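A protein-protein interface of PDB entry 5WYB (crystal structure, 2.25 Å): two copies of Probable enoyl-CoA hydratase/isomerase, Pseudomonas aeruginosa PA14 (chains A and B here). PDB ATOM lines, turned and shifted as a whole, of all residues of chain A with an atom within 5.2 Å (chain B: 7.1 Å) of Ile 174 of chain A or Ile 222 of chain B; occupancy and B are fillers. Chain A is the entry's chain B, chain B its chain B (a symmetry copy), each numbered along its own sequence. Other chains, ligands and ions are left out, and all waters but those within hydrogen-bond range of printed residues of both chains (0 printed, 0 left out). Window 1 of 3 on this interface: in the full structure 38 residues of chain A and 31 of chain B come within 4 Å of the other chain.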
ATOM      1  N   LEU A 144     -16.824  34.582  -8.206  1.00  0.00           N
ATOM      2  CA  LEU A 144     -17.315  34.559  -9.582  1.00  0.00           C
ATOM      3  C   LEU A 144     -18.799  34.236  -9.495  1.00  0.00           C
ATOM      4  O   LEU A 144     -19.194  33.063  -9.533  1.00  0.00           O
ATOM      5  CB  LEU A 144     -16.562  33.541 -10.431  1.00  0.00           C
ATOM      6  CG  LEU A 144     -15.072  33.800 -10.659  1.00  0.00           C
ATOM      7  CD1 LEU A 144     -14.465  32.692 -11.494  1.00  0.00           C
ATOM      8  CD2 LEU A 144     -14.846  35.154 -11.318  1.00  0.00           C
ATOM      9  N   ALA A 147     -23.132  32.713 -12.390  1.00  0.00           N
ATOM     10  CA  ALA A 147     -24.205  31.728 -12.411  1.00  0.00           C
ATOM     11  C   ALA A 147     -25.426  32.172 -11.619  1.00  0.00           C
ATOM     12  O   ALA A 147     -26.511  31.622 -11.821  1.00  0.00           O
ATOM     13  CB  ALA A 147     -23.702  30.392 -11.868  1.00  0.00           C
ATOM     14  N   LEU A 151     -25.533  33.525 -15.958  1.00  0.00           N
ATOM     15  CA  LEU A 151     -24.448  33.744 -16.901  1.00  0.00           C
ATOM     16  C   LEU A 151     -23.238  32.927 -16.477  1.00  0.00           C
ATOM     17  O   LEU A 151     -23.390  31.936 -15.761  1.00  0.00           O
ATOM     18  CB  LEU A 151     -24.121  35.232 -17.004  1.00  0.00           C
ATOM     19  CG  LEU A 151     -25.283  36.076 -17.539  1.00  0.00           C
ATOM     20  CD1 LEU A 151     -24.893  37.520 -17.715  1.00  0.00           C
ATOM     21  CD2 LEU A 151     -25.795  35.508 -18.856  1.00  0.00           C
ATOM     22  N   LEU A 152     -22.047  33.305 -16.923  1.00  0.00           N
ATOM     23  CA  LEU A 152     -20.846  32.545 -16.602  1.00  0.00           C
ATOM     24  C   LEU A 152     -19.652  33.468 -16.685  1.00  0.00           C
ATOM     25  O   LEU A 152     -19.736  34.543 -17.293  1.00  0.00           O
ATOM     26  CB  LEU A 152     -20.677  31.339 -17.541  1.00  0.00           C
ATOM     27  CG  LEU A 152     -20.412  31.472 -19.044  1.00  0.00           C
ATOM     28  CD1 LEU A 152     -18.975  31.840 -19.342  1.00  0.00           C
ATOM     29  CD2 LEU A 152     -20.765  30.166 -19.737  1.00  0.00           C
ATOM     30  N   PRO A 153     -18.509  33.092 -16.082  1.00  0.00           N
ATOM     31  CA  PRO A 153     -17.284  33.882 -16.250  1.00  0.00           C
ATOM     32  C   PRO A 153     -16.714  33.730 -17.654  1.00  0.00           C
ATOM     33  O   PRO A 153     -16.073  32.719 -17.958  1.00  0.00           O
ATOM     34  CB  PRO A 153     -16.334  33.297 -15.197  1.00  0.00           C
ATOM     35  CG  PRO A 153     -17.172  32.450 -14.315  1.00  0.00           C
ATOM     36  CD  PRO A 153     -18.307  31.974 -15.143  1.00  0.00           C
ATOM     37  N   GLY A 157     -12.576  32.731 -16.644  1.00  0.00           N
ATOM     38  CA  GLY A 157     -12.736  32.271 -15.274  1.00  0.00           C
ATOM     39  C   GLY A 157     -12.981  30.780 -15.171  1.00  0.00           C
ATOM     40  O   GLY A 157     -12.502  30.129 -14.237  1.00  0.00           O
ATOM     41  N   THR A 158     -13.714  30.211 -16.133  1.00  0.00           N
ATOM     42  CA  THR A 158     -14.022  28.787 -16.077  1.00  0.00           C
ATOM     43  C   THR A 158     -12.787  27.928 -16.273  1.00  0.00           C
ATOM     44  O   THR A 158     -12.809  26.746 -15.923  1.00  0.00           O
ATOM     45  CB  THR A 158     -15.083  28.424 -17.115  1.00  0.00           C
ATOM     46  OG1 THR A 158     -14.595  28.716 -18.430  1.00  0.00           O
ATOM     47  CG2 THR A 158     -16.352  29.212 -16.873  1.00  0.00           C
ATOM     48  N   LEU A 161      -9.639  29.715 -12.954  1.00  0.00           N
ATOM     49  CA  LEU A 161      -9.869  29.447 -11.534  1.00  0.00           C
ATOM     50  C   LEU A 161      -9.532  28.011 -11.144  1.00  0.00           C
ATOM     51  O   LEU A 161      -8.718  27.827 -10.233  1.00  0.00           O
ATOM     52  CB  LEU A 161     -11.304  29.816 -11.141  1.00  0.00           C
ATOM     53  CG  LEU A 161     -11.627  29.706  -9.645  1.00  0.00           C
ATOM     54  CD1 LEU A 161     -10.728  30.619  -8.822  1.00  0.00           C
ATOM     55  CD2 LEU A 161     -13.092  30.015  -9.364  1.00  0.00           C
ATOM     56  N   TRP A 169     -12.593  23.578  -5.298  1.00  0.00           N
ATOM     57  CA  TRP A 169     -12.813  24.944  -4.844  1.00  0.00           C
ATOM     58  C   TRP A 169     -13.337  25.821  -5.968  1.00  0.00           C
ATOM     59  O   TRP A 169     -14.107  26.758  -5.725  1.00  0.00           O
ATOM     60  CB  TRP A 169     -11.531  25.521  -4.247  1.00  0.00           C
ATOM     61  CG  TRP A 169     -11.513  25.347  -2.765  1.00  0.00           C
ATOM     62  CD1 TRP A 169     -10.814  24.420  -2.051  1.00  0.00           C
ATOM     63  CD2 TRP A 169     -12.273  26.097  -1.816  1.00  0.00           C
ATOM     64  NE1 TRP A 169     -11.079  24.559  -0.712  1.00  0.00           N
ATOM     65  CE2 TRP A 169     -11.973  25.584  -0.543  1.00  0.00           C
ATOM     66  CE3 TRP A 169     -13.171  27.162  -1.920  1.00  0.00           C
ATOM     67  CZ2 TRP A 169     -12.541  26.097   0.618  1.00  0.00           C
ATOM     68  CZ3 TRP A 169     -13.736  27.669  -0.771  1.00  0.00           C
ATOM     69  CH2 TRP A 169     -13.419  27.137   0.483  1.00  0.00           C
ATOM     70  N   ALA A 170     -12.952  25.517  -7.207  1.00  0.00           N
ATOM     71  CA  ALA A 170     -13.401  26.323  -8.331  1.00  0.00           C
ATOM     72  C   ALA A 170     -14.909  26.239  -8.508  1.00  0.00           C
ATOM     73  O   ALA A 170     -15.565  27.251  -8.784  1.00  0.00           O
ATOM     74  CB  ALA A 170     -12.691  25.887  -9.606  1.00  0.00           C
ATOM     75  N   LYS A 171     -15.483  25.050  -8.355  1.00  0.00           N
ATOM     76  CA  LYS A 171     -16.931  24.973  -8.478  1.00  0.00           C
ATOM     77  C   LYS A 171     -17.634  25.280  -7.170  1.00  0.00           C
ATOM     78  O   LYS A 171     -18.840  25.550  -7.175  1.00  0.00           O
ATOM     79  CB  LYS A 171     -17.364  23.612  -9.027  1.00  0.00           C
ATOM     80  CG  LYS A 171     -16.654  22.407  -8.500  1.00  0.00           C
ATOM     81  CD  LYS A 171     -16.958  21.199  -9.373  1.00  0.00           C
ATOM     82  CE  LYS A 171     -16.091  21.138 -10.619  1.00  0.00           C
ATOM     83  NZ  LYS A 171     -16.119  19.759 -11.181  1.00  0.00           N
ATOM     84  N   ARG A 172     -16.895  25.367  -6.080  1.00  0.00           N
ATOM     85  CA  ARG A 172     -17.447  25.842  -4.860  1.00  0.00           C
ATOM     86  C   ARG A 172     -17.719  27.329  -5.081  1.00  0.00           C
ATOM     87  O   ARG A 172     -18.727  27.816  -4.677  1.00  0.00           O
ATOM     88  CB  ARG A 172     -16.537  25.602  -3.686  1.00  0.00           C
ATOM     89  CG  ARG A 172     -17.255  25.020  -2.534  1.00  0.00           C
ATOM     90  CD  ARG A 172     -16.470  25.073  -1.264  1.00  0.00           C
ATOM     91  NE  ARG A 172     -17.230  25.719  -0.231  1.00  0.00           N
ATOM     92  CZ  ARG A 172     -16.960  25.630   1.047  1.00  0.00           C
ATOM     93  NH1 ARG A 172     -15.960  24.905   1.457  1.00  0.00           N
ATOM     94  NH2 ARG A 172     -17.715  26.261   1.894  1.00  0.00           N
ATOM     95  N   MET A 173     -16.825  28.018  -5.772  1.00  0.00           N
ATOM     96  CA  MET A 173     -16.982  29.450  -6.001  1.00  0.00           C
ATOM     97  C   MET A 173     -17.982  29.743  -7.120  1.00  0.00           C
ATOM     98  O   MET A 173     -18.819  30.645  -6.991  1.00  0.00           O
ATOM     99  CB  MET A 173     -15.621  30.079  -6.304  1.00  0.00           C
ATOM    100  CG  MET A 173     -14.714  30.165  -5.089  1.00  0.00           C
ATOM    101  SD  MET A 173     -13.100  30.886  -5.412  1.00  0.00           S
ATOM    102  CE  MET A 173     -13.504  32.604  -5.670  1.00  0.00           C
ATOM    103  N   ILE A 174     -17.911  28.997  -8.228  1.00  0.00           N
ATOM    104  CA  ILE A 174     -18.721  29.319  -9.405  1.00  0.00           C
ATOM    105  C   ILE A 174     -20.093  28.666  -9.324  1.00  0.00           C
ATOM    106  O   ILE A 174     -21.126  29.313  -9.532  1.00  0.00           O
ATOM    107  CB  ILE A 174     -17.995  28.888 -10.694  1.00  0.00           C
ATOM    108  CG1 ILE A 174     -16.702  29.675 -10.884  1.00  0.00           C
ATOM    109  CG2 ILE A 174     -18.906  29.067 -11.887  1.00  0.00           C
ATOM    110  CD1 ILE A 174     -15.724  28.967 -11.774  1.00  0.00           C
ATOM    111  N   LEU A 175     -20.119  27.363  -9.052  1.00  0.00           N
ATOM    112  CA  LEU A 175     -21.370  26.614  -9.094  1.00  0.00           C
ATOM    113  C   LEU A 175     -22.190  26.822  -7.828  1.00  0.00           C
ATOM    114  O   LEU A 175     -23.422  26.735  -7.861  1.00  0.00           O
ATOM    115  CB  LEU A 175     -21.073  25.132  -9.314  1.00  0.00           C
ATOM    116  CG  LEU A 175     -21.086  24.605 -10.752  1.00  0.00           C
ATOM    117  CD1 LEU A 175     -20.624  25.646 -11.774  1.00  0.00           C
ATOM    118  CD2 LEU A 175     -20.232  23.368 -10.849  1.00  0.00           C
ATOM    119  N   CYS A 176     -21.532  27.101  -6.705  1.00  0.00           N
ATOM    120  CA  CYS A 176     -22.232  27.326  -5.448  1.00  0.00           C
ATOM    121  C   CYS A 176     -22.313  28.796  -5.066  1.00  0.00           C
ATOM    122  O   CYS A 176     -22.974  29.119  -4.073  1.00  0.00           O
ATOM    123  CB  CYS A 176     -21.561  26.541  -4.319  1.00  0.00           C
ATOM    124  SG  CYS A 176     -21.493  24.759  -4.599  1.00  0.00           S
ATOM    125  N   ASN A 177     -21.666  29.682  -5.820  1.00  0.00           N
ATOM    126  CA  ASN A 177     -21.691  31.124  -5.591  1.00  0.00           C
ATOM    127  C   ASN A 177     -21.080  31.522  -4.248  1.00  0.00           C
ATOM    128  O   ASN A 177     -21.399  32.584  -3.711  1.00  0.00           O
ATOM    129  CB  ASN A 177     -23.118  31.676  -5.706  1.00  0.00           C
ATOM    130  CG  ASN A 177     -23.152  33.183  -5.866  1.00  0.00           C
ATOM    131  OD1 ASN A 177     -22.123  33.815  -6.096  1.00  0.00           O
ATOM    132  ND2 ASN A 177     -24.340  33.767  -5.739  1.00  0.00           N
ATOM    133  N   GLN B 214     -28.994  29.165  -7.731  1.00  0.00           N
ATOM    134  CA  GLN B 214     -28.394  29.555  -8.982  1.00  0.00           C
ATOM    135  C   GLN B 214     -29.152  29.036 -10.176  1.00  0.00           C
ATOM    136  O   GLN B 214     -29.864  28.103 -10.080  1.00  0.00           O
ATOM    137  CB  GLN B 214     -26.997  29.037  -9.068  1.00  0.00           C
ATOM    138  CG  GLN B 214     -25.987  30.086  -8.774  1.00  0.00           C
ATOM    139  CD  GLN B 214     -25.890  30.346  -7.324  1.00  0.00           C
ATOM    140  OE1 GLN B 214     -25.420  29.516  -6.598  1.00  0.00           O
ATOM    141  NE2 GLN B 214     -26.320  31.498  -6.897  1.00  0.00           N
ATOM    142  N   SER B 215     -28.991  29.684 -11.308  1.00  0.00           N
ATOM    143  CA  SER B 215     -29.654  29.214 -12.514  1.00  0.00           C
ATOM    144  C   SER B 215     -29.230  27.783 -12.815  1.00  0.00           C
ATOM    145  O   SER B 215     -28.030  27.524 -12.981  1.00  0.00           O
ATOM    146  CB  SER B 215     -29.319  30.125 -13.687  1.00  0.00           C
ATOM    147  OG  SER B 215     -29.813  29.601 -14.907  1.00  0.00           O
ATOM    148  N   PRO B 216     -30.159  26.827 -12.862  1.00  0.00           N
ATOM    149  CA  PRO B 216     -29.764  25.454 -13.216  1.00  0.00           C
ATOM    150  C   PRO B 216     -29.157  25.350 -14.601  1.00  0.00           C
ATOM    151  O   PRO B 216     -28.167  24.636 -14.789  1.00  0.00           O
ATOM    152  CB  PRO B 216     -31.082  24.674 -13.115  1.00  0.00           C
ATOM    153  CG  PRO B 216     -31.957  25.511 -12.247  1.00  0.00           C
ATOM    154  CD  PRO B 216     -31.588  26.928 -12.537  1.00  0.00           C
ATOM    155  N   VAL B 217     -29.711  26.063 -15.580  1.00  0.00           N
ATOM    156  CA  VAL B 217     -29.169  25.972 -16.932  1.00  0.00           C
ATOM    157  C   VAL B 217     -27.759  26.539 -16.976  1.00  0.00           C
ATOM    158  O   VAL B 217     -26.946  26.137 -17.814  1.00  0.00           O
ATOM    159  CB  VAL B 217     -30.109  26.664 -17.941  1.00  0.00           C
ATOM    160  CG1 VAL B 217     -30.014  28.168 -17.827  1.00  0.00           C
ATOM    161  CG2 VAL B 217     -29.792  26.212 -19.355  1.00  0.00           C
ATOM    162  N   ALA B 218     -27.429  27.453 -16.062  1.00  0.00           N
ATOM    163  CA  ALA B 218     -26.059  27.940 -15.991  1.00  0.00           C
ATOM    164  C   ALA B 218     -25.144  26.899 -15.364  1.00  0.00           C
ATOM    165  O   ALA B 218     -24.001  26.733 -15.796  1.00  0.00           O
ATOM    166  CB  ALA B 218     -26.002  29.250 -15.209  1.00  0.00           C
ATOM    167  N   ILE B 219     -25.629  26.189 -14.346  1.00  0.00           N
ATOM    168  CA  ILE B 219     -24.817  25.142 -13.735  1.00  0.00           C
ATOM    169  C   ILE B 219     -24.498  24.060 -14.755  1.00  0.00           C
ATOM    170  O   ILE B 219     -23.350  23.614 -14.877  1.00  0.00           O
ATOM    171  CB  ILE B 219     -25.534  24.560 -12.504  1.00  0.00           C
ATOM    172  CG1 ILE B 219     -25.781  25.650 -11.460  1.00  0.00           C
ATOM    173  CG2 ILE B 219     -24.727  23.426 -11.911  1.00  0.00           C
ATOM    174  CD1 ILE B 219     -24.524  26.338 -10.989  1.00  0.00           C
ATOM    175  N   ARG B 220     -25.506  23.634 -15.517  1.00  0.00           N
ATOM    176  CA  ARG B 220     -25.314  22.541 -16.461  1.00  0.00           C
ATOM    177  C   ARG B 220     -24.327  22.918 -17.557  1.00  0.00           C
ATOM    178  O   ARG B 220     -23.571  22.067 -18.032  1.00  0.00           O
ATOM    179  CB  ARG B 220     -26.652  22.137 -17.067  1.00  0.00           C
ATOM    180  CG  ARG B 220     -27.736  21.968 -16.046  1.00  0.00           C
ATOM    181  CD  ARG B 220     -28.900  21.244 -16.644  1.00  0.00           C
ATOM    182  NE  ARG B 220     -30.182  21.900 -16.403  1.00  0.00           N
ATOM    183  CZ  ARG B 220     -31.031  21.574 -15.434  1.00  0.00           C
ATOM    184  NH1 ARG B 220     -30.738  20.598 -14.583  1.00  0.00           N
ATOM    185  NH2 ARG B 220     -32.179  22.226 -15.316  1.00  0.00           N
ATOM    186  N   THR B 221     -24.372  24.149 -18.017  1.00  0.00           N
ATOM    187  CA  THR B 221     -23.419  24.622 -18.997  1.00  0.00           C
ATOM    188  C   THR B 221     -22.003  24.879 -18.481  1.00  0.00           C
ATOM    189  O   THR B 221     -21.050  24.613 -19.148  1.00  0.00           O
ATOM    190  CB  THR B 221     -23.928  25.775 -19.848  1.00  0.00           C
ATOM    191  OG1 THR B 221     -24.690  26.635 -19.050  1.00  0.00           O
ATOM    192  CG2 THR B 221     -24.795  25.250 -20.841  1.00  0.00           C
ATOM    193  N   ILE B 222     -21.908  25.443 -17.288  1.00  0.00           N
ATOM    194  CA  ILE B 222     -20.629  25.761 -16.699  1.00  0.00           C
ATOM    195  C   ILE B 222     -19.778  24.574 -16.270  1.00  0.00           C
ATOM    196  O   ILE B 222     -18.620  24.537 -16.519  1.00  0.00           O
ATOM    197  CB  ILE B 222     -20.729  26.793 -15.581  1.00  0.00           C
ATOM    198  CG1 ILE B 222     -21.387  28.070 -16.065  1.00  0.00           C
ATOM    199  CG2 ILE B 222     -19.363  27.107 -15.026  1.00  0.00           C
ATOM    200  CD1 ILE B 222     -21.670  29.085 -15.003  1.00  0.00           C
ATOM    201  N   LYS B 223     -20.400  23.586 -15.674  1.00  0.00           N
ATOM    202  CA  LYS B 223     -19.676  22.471 -15.140  1.00  0.00           C
ATOM    203  C   LYS B 223     -18.827  21.744 -16.129  1.00  0.00           C
ATOM    204  O   LYS B 223     -17.704  21.488 -15.816  1.00  0.00           O
ATOM    205  CB  LYS B 223     -20.616  21.559 -14.413  1.00  0.00           C
ATOM    206  CG  LYS B 223     -20.055  20.263 -13.976  1.00  0.00           C
ATOM    207  CD  LYS B 223     -21.205  19.412 -13.520  1.00  0.00           C
ATOM    208  CE  LYS B 223     -20.900  18.540 -12.349  1.00  0.00           C
ATOM    209  NZ  LYS B 223     -19.960  17.520 -12.740  1.00  0.00           N
ATOM    210  N   PRO B 224     -19.302  21.458 -17.333  1.00  0.00           N
ATOM    211  CA  PRO B 224     -18.383  20.815 -18.281  1.00  0.00           C
ATOM    212  C   PRO B 224     -17.195  21.697 -18.621  1.00  0.00           C
ATOM    213  O   PRO B 224     -16.129  21.201 -18.871  1.00  0.00           O
ATOM    214  CB  PRO B 224     -19.230  20.598 -19.502  1.00  0.00           C
ATOM    215  CG  PRO B 224     -20.567  20.421 -18.988  1.00  0.00           C
ATOM    216  CD  PRO B 224     -20.662  21.513 -18.008  1.00  0.00           C
ATOM    217  N   LEU B 225     -17.406  23.002 -18.647  1.00  0.00           N
ATOM    218  CA  LEU B 225     -16.329  23.940 -18.903  1.00  0.00           C
ATOM    219  C   LEU B 225     -15.251  23.869 -17.809  1.00  0.00           C
ATOM    220  O   LEU B 225     -14.104  23.915 -18.078  1.00  0.00           O
ATOM    221  CB  LEU B 225     -16.839  25.361 -19.049  1.00  0.00           C
ATOM    222  CG  LEU B 225     -17.527  25.775 -20.344  1.00  0.00           C
ATOM    223  CD1 LEU B 225     -17.966  27.211 -20.362  1.00  0.00           C
ATOM    224  CD2 LEU B 225     -16.622  25.486 -21.508  1.00  0.00           C
ATOM    225  N   ILE B 226     -15.664  23.751 -16.566  1.00  0.00           N
ATOM    226  CA  ILE B 226     -14.711  23.660 -15.466  1.00  0.00           C
ATOM    227  C   ILE B 226     -13.880  22.391 -15.590  1.00  0.00           C
ATOM    228  O   ILE B 226     -12.661  22.410 -15.394  1.00  0.00           O
ATOM    229  CB  ILE B 226     -15.442  23.739 -14.110  1.00  0.00           C
ATOM    230  CG1 ILE B 226     -16.157  25.081 -13.968  1.00  0.00           C
ATOM    231  CG2 ILE B 226     -14.467  23.570 -12.973  1.00  0.00           C
ATOM    232  CD1 ILE B 226     -16.893  25.246 -12.658  1.00  0.00           C
ATOM    233  N   GLN B 227     -14.513  21.280 -15.942  1.00  0.00           N
ATOM    234  CA  GLN B 227     -13.790  20.027 -16.128  1.00  0.00           C
ATOM    235  C   GLN B 227     -13.073  19.936 -17.476  1.00  0.00           C
ATOM    236  O   GLN B 227     -12.568  18.862 -17.812  1.00  0.00           O
ATOM    237  CB  GLN B 227     -14.749  18.853 -15.963  1.00  0.00           C
ATOM    238  CG  GLN B 227     -15.368  18.798 -14.596  1.00  0.00           C
ATOM    239  CD  GLN B 227     -16.526  17.847 -14.533  1.00  0.00           C
ATOM    240  OE1 GLN B 227     -16.794  17.245 -13.496  1.00  0.00           O
ATOM    241  NE2 GLN B 227     -17.232  17.710 -15.644  1.00  0.00           N
ATOM    242  N   GLY B 228     -12.990  21.036 -18.228  1.00  0.00           N
ATOM    243  CA  GLY B 228     -12.399  20.985 -19.555  1.00  0.00           C
ATOM    244  C   GLY B 228     -10.962  20.503 -19.571  1.00  0.00           C
ATOM    245  O   GLY B 228     -10.556  19.794 -20.494  1.00  0.00           O
ATOM    246  N   ARG B 244     -20.633  29.619 -25.196  1.00  0.00           N
ATOM    247  CA  ARG B 244     -21.649  29.219 -24.231  1.00  0.00           C
ATOM    248  C   ARG B 244     -22.091  30.380 -23.351  1.00  0.00           C
ATOM    249  O   ARG B 244     -23.204  30.351 -22.820  1.00  0.00           O
ATOM    250  CB  ARG B 244     -21.130  28.061 -23.385  1.00  0.00           C
ATOM    251  CG  ARG B 244     -20.895  26.806 -24.201  1.00  0.00           C
ATOM    252  CD  ARG B 244     -20.150  25.739 -23.425  1.00  0.00           C
ATOM    253  NE  ARG B 244     -21.037  24.853 -22.677  1.00  0.00           N
ATOM    254  CZ  ARG B 244     -20.757  23.582 -22.405  1.00  0.00           C
ATOM    255  NH1 ARG B 244     -19.620  23.048 -22.835  1.00  0.00           N
ATOM    256  NH2 ARG B 244     -21.615  22.840 -21.721  1.00  0.00           N
ATOM    257  N   LEU B 248     -25.953  31.366 -23.011  1.00  0.00           N
ATOM    258  CA  LEU B 248     -26.638  31.679 -21.764  1.00  0.00           C
ATOM    259  C   LEU B 248     -27.272  33.060 -21.796  1.00  0.00           C
ATOM    260  O   LEU B 248     -28.328  33.262 -21.190  1.00  0.00           O
ATOM    261  CB  LEU B 248     -25.673  31.569 -20.583  1.00  0.00           C
ATOM    262  CG  LEU B 248     -25.289  30.158 -20.132  1.00  0.00           C
ATOM    263  CD1 LEU B 248     -24.367  30.226 -18.938  1.00  0.00           C
ATOM    264  CD2 LEU B 248     -26.524  29.321 -19.813  1.00  0.00           C
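ND2 of Asn 177 of chain A sits close to NE2 of Gln 214 of chain B (3.2 Å). The side-chain amino group (NZ) of Lys 171 of chain A is in hydrogen-bond range of the side-chain amide oxygen (OE1) of Gln 227 of chain B. O of Ala 147 of chain A sits at hydrogen-bond distance from N of Ser 215 of chain B (3.2 Å).
The side-chain hydroxyl (OG) of Ser 215 of chain B is in hydrogen-bond range of the backbone NH (N) of Ala 218 of chain B. The backbone carbonyl oxygen (O) of Ala 218 of chain B is in hydrogen-bond range of the side-chain hydroxyl (OG1) of Thr 221 of chain B, 3.3 Å away. The backbone carbonyl oxygen (O) of Lys 171 of chain A sits at hydrogen-bond distance from the backbone NH (N) of Cys 176 of chain A, at 3.1 Å. The guanidinium group (NH2) of Arg 244 of chain B sits at hydrogen-bond distance from the backbone carbonyl oxygen (O) of Thr 221 of chain B (3.2 Å). The side-chain amino group (NZ) of Lys 223 of chain B lies within hydrogen-bond range of the side-chain amide oxygen (OE1) of Gln 227 of chain B, at 3.3 Å.
Gln 214 of chain B touches Ala 147 of chain A. Ala 147 of chain A touches Ile 222 of chain B. Leu 151 of chain A touches Ile 222 of chain B. Leu 151 of chain A touches Leu 248 of chain B. CD1 of Ile 222 of chain B touches CB of Leu 152 of chain A (3.5 Å). Arg 244 of chain B touches Leu 152 of chain A. Leu 152 of chain A touches Leu 248 of chain B (CD2 to CD1, 3.7 Å). Leu 175 of chain A touches Ile 219 of chain B (O to CD1, 3.3 Å). CG2 of Ile 222 of chain B touches CD1 of Leu 175 of chain A (3.8 Å). CD1 of Ile 226 of chain B touches CD1 of Leu 175 of chain A, at 3.9 Å.
Leu 144 of chain A touches none of the printed residues of chain B. Of the printed residues of chain B, Ala 147 of chain A touches Gln 214, Ser 215 and Ile 222. Of the printed residues of chain B, Leu 151 of chain A touches Ala 218, Ile 222 and Leu 248. Of the printed residues of chain B, Leu 152 of chain A touches Ile 222, Arg 244 and Leu 248. Of the printed residues of chain B, Ile 174 of chain A touches Ile 222 (3.7 Å) and Ile 226 (3.999 Å). Ile 222 of chain B touches five residues of chain A. Pro 224 of chain B touches none of the printed residues of chain A. Printed residues of chain A within 4 Å of Arg 244 of chain B: Leu 152.
Of the 17 printed residues of chain A, 9 touch a printed residue of chain B. Printed residues of chain A that touch a printed residue of chain B: Ala 147, Leu 151, Leu 152, Thr 158, Lys 171, Ile 174, Leu 175, Cys 176 and Asn 177. Hydrophobic or aromatic side chains of chain A that line the printed part of chain B: Ala 147, Leu 152, Ile 174 and Leu 175. Among the printed residues, no Asp or Glu carboxylate lies within 4 Å of a Lys or Arg side-chain nitrogen of the other chain.
No position is printed for both chains. Of the 21 pairs that touch across the chains among the printed residues, none has its exchanged pair printed and touching as well.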
